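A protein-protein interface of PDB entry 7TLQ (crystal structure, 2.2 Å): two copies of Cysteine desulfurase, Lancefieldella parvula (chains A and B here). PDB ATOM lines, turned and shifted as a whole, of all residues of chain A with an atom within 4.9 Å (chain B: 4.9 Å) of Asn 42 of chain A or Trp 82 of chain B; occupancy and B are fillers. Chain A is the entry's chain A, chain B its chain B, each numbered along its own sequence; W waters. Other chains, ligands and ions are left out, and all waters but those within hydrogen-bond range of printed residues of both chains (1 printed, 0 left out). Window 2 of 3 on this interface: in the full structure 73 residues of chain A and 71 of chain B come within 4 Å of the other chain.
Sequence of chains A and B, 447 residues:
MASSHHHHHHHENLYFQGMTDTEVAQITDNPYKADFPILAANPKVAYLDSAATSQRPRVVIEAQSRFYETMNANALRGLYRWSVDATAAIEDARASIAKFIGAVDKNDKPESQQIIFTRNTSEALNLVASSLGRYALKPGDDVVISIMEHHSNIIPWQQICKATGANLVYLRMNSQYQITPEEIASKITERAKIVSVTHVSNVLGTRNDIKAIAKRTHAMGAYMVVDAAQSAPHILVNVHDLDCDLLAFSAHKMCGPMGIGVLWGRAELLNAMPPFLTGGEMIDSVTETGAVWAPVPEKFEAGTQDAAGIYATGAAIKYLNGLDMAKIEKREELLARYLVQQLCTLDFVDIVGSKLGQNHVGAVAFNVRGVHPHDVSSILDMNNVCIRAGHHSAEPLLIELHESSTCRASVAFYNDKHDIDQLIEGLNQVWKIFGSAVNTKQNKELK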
ATOM      1  N   PRO A  37       7.557   3.014 -24.277  1.00  0.00           N
ATOM      2  CA  PRO A  37       7.464   3.358 -25.707  1.00  0.00           C
ATOM      3  C   PRO A  37       7.839   4.793 -26.044  1.00  0.00           C
ATOM      4  O   PRO A  37       8.524   5.018 -27.049  1.00  0.00           O
ATOM      5  CB  PRO A  37       5.991   3.076 -26.027  1.00  0.00           C
ATOM      6  CG  PRO A  37       5.609   2.002 -25.075  1.00  0.00           C
ATOM      7  CD  PRO A  37       6.369   2.282 -23.805  1.00  0.00           C
ATOM      8  N   ILE A  38       7.408   5.771 -25.243  1.00  0.00           N
ATOM      9  CA  ILE A  38       7.708   7.163 -25.572  1.00  0.00           C
ATOM     10  C   ILE A  38       9.205   7.430 -25.493  1.00  0.00           C
ATOM     11  O   ILE A  38       9.735   8.261 -26.240  1.00  0.00           O
ATOM     12  CB  ILE A  38       6.907   8.122 -24.665  1.00  0.00           C
ATOM     13  CG1 ILE A  38       6.801   9.504 -25.314  1.00  0.00           C
ATOM     14  CG2 ILE A  38       7.540   8.234 -23.286  1.00  0.00           C
ATOM     15  CD1 ILE A  38       5.944  10.481 -24.538  1.00  0.00           C
ATOM     16  N   LEU A  39       9.915   6.724 -24.609  1.00  0.00           N
ATOM     17  CA  LEU A  39      11.352   6.933 -24.480  1.00  0.00           C
ATOM     18  C   LEU A  39      12.117   6.212 -25.581  1.00  0.00           C
ATOM     19  O   LEU A  39      13.105   6.741 -26.103  1.00  0.00           O
ATOM     20  CB  LEU A  39      11.828   6.471 -23.103  1.00  0.00           C
ATOM     21  CG  LEU A  39      11.264   7.237 -21.904  1.00  0.00           C
ATOM     22  CD1 LEU A  39      11.846   6.706 -20.602  1.00  0.00           C
ATOM     23  CD2 LEU A  39      11.527   8.729 -22.046  1.00  0.00           C
ATOM     24  N   ALA A  40      11.674   5.007 -25.944  1.00  0.00           N
ATOM     25  CA  ALA A  40      12.302   4.290 -27.049  1.00  0.00           C
ATOM     26  C   ALA A  40      12.095   5.023 -28.368  1.00  0.00           C
ATOM     27  O   ALA A  40      12.999   5.072 -29.210  1.00  0.00           O
ATOM     28  CB  ALA A  40      11.749   2.868 -27.132  1.00  0.00           C
ATOM     29  N   ALA A  41      10.910   5.605 -28.562  1.00  0.00           N
ATOM     30  CA  ALA A  41      10.599   6.304 -29.802  1.00  0.00           C
ATOM     31  C   ALA A  41      11.256   7.675 -29.893  1.00  0.00           C
ATOM     32  O   ALA A  41      11.394   8.207 -30.999  1.00  0.00           O
ATOM     33  CB  ALA A  41       9.084   6.455 -29.955  1.00  0.00           C
ATOM     34  N   ASN A  42      11.662   8.256 -28.766  1.00  0.00           N
ATOM     35  CA  ASN A  42      12.303   9.571 -28.731  1.00  0.00           C
ATOM     36  C   ASN A  42      13.614   9.457 -27.966  1.00  0.00           C
ATOM     37  O   ASN A  42      13.736   9.943 -26.836  1.00  0.00           O
ATOM     38  CB  ASN A  42      11.379  10.611 -28.097  1.00  0.00           C
ATOM     39  CG  ASN A  42      10.060  10.745 -28.833  1.00  0.00           C
ATOM     40  OD1 ASN A  42       9.939  11.518 -29.784  1.00  0.00           O
ATOM     41  ND2 ASN A  42       9.061   9.984 -28.397  1.00  0.00           N
ATOM     42  N   PRO A  43      14.629   8.827 -28.567  1.00  0.00           N
ATOM     43  CA  PRO A  43      15.867   8.547 -27.819  1.00  0.00           C
ATOM     44  C   PRO A  43      16.670   9.785 -27.454  1.00  0.00           C
ATOM     45  O   PRO A  43      17.499   9.710 -26.539  1.00  0.00           O
ATOM     46  CB  PRO A  43      16.650   7.637 -28.773  1.00  0.00           C
ATOM     47  CG  PRO A  43      16.168   8.028 -30.131  1.00  0.00           C
ATOM     48  CD  PRO A  43      14.711   8.371 -29.966  1.00  0.00           C
ATOM     49  N   LYS A  44      16.459  10.914 -28.127  1.00  0.00           N
ATOM     50  CA  LYS A  44      17.204  12.128 -27.815  1.00  0.00           C
ATOM     51  C   LYS A  44      16.656  12.870 -26.602  1.00  0.00           C
ATOM     52  O   LYS A  44      17.338  13.762 -26.086  1.00  0.00           O
ATOM     53  CB  LYS A  44      17.211  13.066 -29.024  1.00  0.00           C
ATOM     54  N   VAL A  45      15.464  12.521 -26.132  1.00  0.00           N
ATOM     55  CA  VAL A  45      14.771  13.295 -25.109  1.00  0.00           C
ATOM     56  C   VAL A  45      15.211  12.826 -23.729  1.00  0.00           C
ATOM     57  O   VAL A  45      15.163  11.628 -23.421  1.00  0.00           O
ATOM     58  CB  VAL A  45      13.247  13.174 -25.273  1.00  0.00           C
ATOM     59  CG1 VAL A  45      12.534  13.798 -24.085  1.00  0.00           C
ATOM     60  CG2 VAL A  45      12.804  13.822 -26.576  1.00  0.00           C
ATOM     61  N   TYR A  47      13.990  13.076 -20.240  1.00  0.00           N
ATOM     62  CA  TYR A  47      12.834  13.412 -19.414  1.00  0.00           C
ATOM     63  C   TYR A  47      13.244  13.409 -17.945  1.00  0.00           C
ATOM     64  O   TYR A  47      13.483  12.346 -17.361  1.00  0.00           O
ATOM     65  CB  TYR A  47      11.693  12.430 -19.665  1.00  0.00           C
ATOM     66  CG  TYR A  47      10.423  12.785 -18.927  1.00  0.00           C
ATOM     67  CD1 TYR A  47       9.635  13.853 -19.338  1.00  0.00           C
ATOM     68  CD2 TYR A  47      10.013  12.057 -17.818  1.00  0.00           C
ATOM     69  CE1 TYR A  47       8.475  14.184 -18.666  1.00  0.00           C
ATOM     70  CE2 TYR A  47       8.852  12.381 -17.139  1.00  0.00           C
ATOM     71  CZ  TYR A  47       8.087  13.445 -17.569  1.00  0.00           C
ATOM     72  OH  TYR A  47       6.930  13.777 -16.900  1.00  0.00           O
ATOM     73  N   GLN A  55       6.567   8.355 -16.931  1.00  0.00           N
ATOM     74  CA  GLN A  55       6.280   7.753 -18.218  1.00  0.00           C
ATOM     75  C   GLN A  55       5.637   6.390 -17.995  1.00  0.00           C
ATOM     76  O   GLN A  55       5.707   5.813 -16.906  1.00  0.00           O
ATOM     77  CB  GLN A  55       7.548   7.627 -19.063  1.00  0.00           C
ATOM     78  CG  GLN A  55       8.146   8.960 -19.500  1.00  0.00           C
ATOM     79  CD  GLN A  55       7.109   9.932 -20.046  1.00  0.00           C
ATOM     80  OE1 GLN A  55       6.182   9.541 -20.757  1.00  0.00           O
ATOM     81  NE2 GLN A  55       7.268  11.208 -19.717  1.00  0.00           N
ATOM     82  N   CYS A 386      13.546  17.957 -20.415  1.00  0.00           N
ATOM     83  CA  CYS A 386      12.264  18.286 -19.801  1.00  0.00           C
ATOM     84  C   CYS A 386      12.464  18.446 -18.299  1.00  0.00           C
ATOM     85  O   CYS A 386      12.744  17.469 -17.597  1.00  0.00           O
ATOM     86  CB  CYS A 386      11.223  17.208 -20.099  1.00  0.00           C
ATOM     87  SG  CYS A 386      11.119  16.719 -21.836  1.00  0.00           S
ATOM     88  N   THR B  70       2.801   8.979 -26.865  1.00  0.00           N
ATOM     89  CA  THR B  70       3.311  10.065 -27.698  1.00  0.00           C
ATOM     90  C   THR B  70       3.362  11.430 -27.014  1.00  0.00           C
ATOM     91  O   THR B  70       4.202  12.261 -27.378  1.00  0.00           O
ATOM     92  CB  THR B  70       2.487  10.172 -28.986  1.00  0.00           C
ATOM     93  OG1 THR B  70       1.161  10.620 -28.678  1.00  0.00           O
ATOM     94  CG2 THR B  70       2.426   8.830 -29.710  1.00  0.00           C
ATOM     95  N   MET B  71       2.490  11.698 -26.046  1.00  0.00           N
ATOM     96  CA  MET B  71       2.482  13.016 -25.410  1.00  0.00           C
ATOM     97  C   MET B  71       2.078  12.909 -23.941  1.00  0.00           C
ATOM     98  O   MET B  71       1.283  13.701 -23.432  1.00  0.00           O
ATOM     99  CB  MET B  71       1.562  13.983 -26.157  1.00  0.00           C
ATOM    100  CG  MET B  71       0.125  13.506 -26.309  1.00  0.00           C
ATOM    101  SD  MET B  71      -0.838  14.548 -27.420  1.00  0.00           S
ATOM    102  CE  MET B  71      -2.107  13.400 -27.945  1.00  0.00           C
ATOM    103  N   ASN B  72       2.641  11.939 -23.228  1.00  0.00           N
ATOM    104  CA  ASN B  72       2.316  11.754 -21.818  1.00  0.00           C
ATOM    105  C   ASN B  72       3.071  12.782 -20.980  1.00  0.00           C
ATOM    106  O   ASN B  72       4.305  12.749 -20.912  1.00  0.00           O
ATOM    107  CB  ASN B  72       2.658  10.336 -21.371  1.00  0.00           C
ATOM    108  CG  ASN B  72       2.514  10.146 -19.873  1.00  0.00           C
ATOM    109  OD1 ASN B  72       1.402  10.074 -19.349  1.00  0.00           O
ATOM    110  ND2 ASN B  72       3.642  10.064 -19.175  1.00  0.00           N
ATOM    111  N   ALA B  73       2.332  13.689 -20.347  1.00  0.00           N
ATOM    112  CA  ALA B  73       2.927  14.734 -19.517  1.00  0.00           C
ATOM    113  C   ALA B  73       1.891  15.360 -18.587  1.00  0.00           C
ATOM    114  O   ALA B  73       0.741  15.569 -18.975  1.00  0.00           O
ATOM    115  CB  ALA B  73       3.568  15.804 -20.387  1.00  0.00           C
ATOM    116  N   TYR B  80       7.905  22.078 -21.781  1.00  0.00           N
ATOM    117  CA  TYR B  80       8.570  21.271 -22.789  1.00  0.00           C
ATOM    118  C   TYR B  80       7.543  20.708 -23.769  1.00  0.00           C
ATOM    119  O   TYR B  80       6.330  20.810 -23.563  1.00  0.00           O
ATOM    120  CB  TYR B  80       9.389  20.152 -22.142  1.00  0.00           C
ATOM    121  CG  TYR B  80       8.712  19.444 -20.991  1.00  0.00           C
ATOM    122  CD1 TYR B  80       7.920  18.324 -21.209  1.00  0.00           C
ATOM    123  CD2 TYR B  80       8.877  19.885 -19.683  1.00  0.00           C
ATOM    124  CE1 TYR B  80       7.306  17.667 -20.159  1.00  0.00           C
ATOM    125  CE2 TYR B  80       8.266  19.236 -18.626  1.00  0.00           C
ATOM    126  CZ  TYR B  80       7.482  18.128 -18.871  1.00  0.00           C
ATOM    127  OH  TYR B  80       6.872  17.480 -17.821  1.00  0.00           O
ATOM    128  N   ARG B  81       8.045  20.100 -24.847  1.00  0.00           N
ATOM    129  CA  ARG B  81       7.189  19.788 -25.989  1.00  0.00           C
ATOM    130  C   ARG B  81       6.008  18.907 -25.598  1.00  0.00           C
ATOM    131  O   ARG B  81       4.867  19.168 -25.996  1.00  0.00           O
ATOM    132  CB  ARG B  81       7.993  19.121 -27.104  1.00  0.00           C
ATOM    133  CG  ARG B  81       7.101  18.805 -28.288  1.00  0.00           C
ATOM    134  CD  ARG B  81       6.707  20.093 -28.995  1.00  0.00           C
ATOM    135  NE  ARG B  81       5.486  19.950 -29.785  1.00  0.00           N
ATOM    136  CZ  ARG B  81       5.424  19.432 -31.007  1.00  0.00           C
ATOM    137  NH1 ARG B  81       6.521  18.986 -31.605  1.00  0.00           N
ATOM    138  NH2 ARG B  81       4.255  19.356 -31.630  1.00  0.00           N
ATOM    139  N   TRP B  82       6.264  17.857 -24.816  1.00  0.00           N
ATOM    140  CA  TRP B  82       5.201  16.915 -24.483  1.00  0.00           C
ATOM    141  C   TRP B  82       4.093  17.584 -23.677  1.00  0.00           C
ATOM    142  O   TRP B  82       2.909  17.278 -23.864  1.00  0.00           O
ATOM    143  CB  TRP B  82       5.781  15.723 -23.724  1.00  0.00           C
ATOM    144  CG  TRP B  82       6.571  14.805 -24.600  1.00  0.00           C
ATOM    145  CD1 TRP B  82       6.491  14.701 -25.959  1.00  0.00           C
ATOM    146  CD2 TRP B  82       7.562  13.858 -24.184  1.00  0.00           C
ATOM    147  NE1 TRP B  82       7.371  13.751 -26.414  1.00  0.00           N
ATOM    148  CE2 TRP B  82       8.041  13.217 -25.345  1.00  0.00           C
ATOM    149  CE3 TRP B  82       8.092  13.490 -22.943  1.00  0.00           C
ATOM    150  CZ2 TRP B  82       9.023  12.229 -25.301  1.00  0.00           C
ATOM    151  CZ3 TRP B  82       9.066  12.508 -22.903  1.00  0.00           C
ATOM    152  CH2 TRP B  82       9.520  11.889 -24.074  1.00  0.00           C
ATOM    153  N   SER B  83       4.455  18.507 -22.783  1.00  0.00           N
ATOM    154  CA  SER B  83       3.445  19.187 -21.980  1.00  0.00           C
ATOM    155  C   SER B  83       2.621  20.152 -22.825  1.00  0.00           C
ATOM    156  O   SER B  83       1.402  20.259 -22.641  1.00  0.00           O
ATOM    157  CB  SER B  83       4.104  19.922 -20.815  1.00  0.00           C
ATOM    158  OG  SER B  83       3.130  20.527 -19.982  1.00  0.00           O
ATOM    159  N   VAL B  84       3.267  20.864 -23.751  1.00  0.00           N
ATOM    160  CA  VAL B  84       2.535  21.765 -24.638  1.00  0.00           C
ATOM    161  C   VAL B  84       1.564  20.978 -25.509  1.00  0.00           C
ATOM    162  O   VAL B  84       0.423  21.402 -25.734  1.00  0.00           O
ATOM    163  CB  VAL B  84       3.515  22.594 -25.488  1.00  0.00           C
ATOM    164  CG1 VAL B  84       2.757  23.490 -26.456  1.00  0.00           C
ATOM    165  CG2 VAL B  84       4.421  23.423 -24.592  1.00  0.00           C
ATOM    166  N   ASP B  85       1.997  19.816 -26.004  1.00  0.00           N
ATOM    167  CA  ASP B  85       1.109  18.977 -26.802  1.00  0.00           C
ATOM    168  C   ASP B  85      -0.055  18.458 -25.968  1.00  0.00           C
ATOM    169  O   ASP B  85      -1.205  18.458 -26.427  1.00  0.00           O
ATOM    170  CB  ASP B  85       1.892  17.812 -27.408  1.00  0.00           C
ATOM    171  CG  ASP B  85       2.846  18.255 -28.498  1.00  0.00           C
ATOM    172  OD1 ASP B  85       2.841  19.456 -28.840  1.00  0.00           O
ATOM    173  OD2 ASP B  85       3.598  17.402 -29.015  1.00  0.00           O
ATOM    174  N   ALA B  86       0.221  18.014 -24.740  1.00  0.00           N
ATOM    175  CA  ALA B  86      -0.846  17.520 -23.876  1.00  0.00           C
ATOM    176  C   ALA B  86      -1.826  18.631 -23.523  1.00  0.00           C
ATOM    177  O   ALA B  86      -3.038  18.399 -23.444  1.00  0.00           O
ATOM    178  CB  ALA B  86      -0.255  16.899 -22.610  1.00  0.00           C
HETATM  179  O   HOH W   1       5.127  15.796 -17.266  1.00  0.00           O
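The side-chain amide nitrogen (ND2) of Asn 72 of chain B sits at hydrogen-bond distance from the side-chain amide oxygen (OE1) of Gln 55 of chain A.
The backbone carbonyl oxygen of Ile 38 of chain A lies within hydrogen-bond range of the side-chain amide nitrogen of Asn 42 of chain A (2.8 Å).
Among the printed residues, merely in contact across the chains: Ile 38 of chain A with Thr 70 of chain B (3.7 Å), Ile 38 of chain A with Met 71 of chain B (3.96 Å), Ile 38 of chain A with Asn 72 of chain B (3.8 Å), Ile 38 of chain A with Trp 82 of chain B (3.5 Å), Asn 42 of chain A with Trp 82 of chain B (3.8 Å), Val 45 of chain A with Trp 82 of chain B (3.6 Å), Tyr 47 of chain A with Tyr 80 of chain B (3.8 Å), Tyr 47 of chain A with Trp 82 of chain B (3.9 Å), Gln 55 of chain A with Trp 82 of chain B (3.9 Å) and Cys 386 of chain A with Tyr 80 of chain B (3.5 Å).
Of the printed residues of chain B, Ile 38 of chain A touches Thr 70, Met 71, Asn 72 and Trp 82.
Of the printed residues of chain B, Gln 55 of chain A touches Asn 72 (3.0 Å) and Trp 82 (3.9 Å).
Printed residues of chain A within 4 Å of Met 71 of chain B: Ile 38.
Printed residues of chain A within 4 Å of Asn 72 of chain B: Ile 38 (3.8 Å) and Gln 55 (3.0 Å).
Trp 82 of chain B touches just these residues of chain A: Ile 38, Asn 42, Val 45, Tyr 47 and Gln 55.
The nearest residue of chain A that does not touch Trp 82 of chain B is Leu 39 of chain A (4.3 Å).
The nearest printed residue of chain B that does not touch Gln 55 of chain A is Ala 73 of chain B (5.6 Å).
Hydrophobic or aromatic side chains of chain B that line the printed part of chain A: Tyr 80 and Trp 82.
Of the 12 printed residues of chain A, 6 touch a printed residue of chain B.
Hydrophobic or aromatic side chains of chain A within 4 Å of the printed part of chain B: Ile 38, Val 45 and Tyr 47.
Along chain A the printed residues that touch a printed residue of chain B span positions 38 to 386.
Among the printed residues, 11 pairs touch across the chains.
No position is printed for both chains.
Water W1 lies within hydrogen-bond range of the side-chain hydroxyl of Tyr 80 of chain B (2.5 Å) and the side-chain hydroxyl of Tyr 47 of chain A (2.7 Å).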
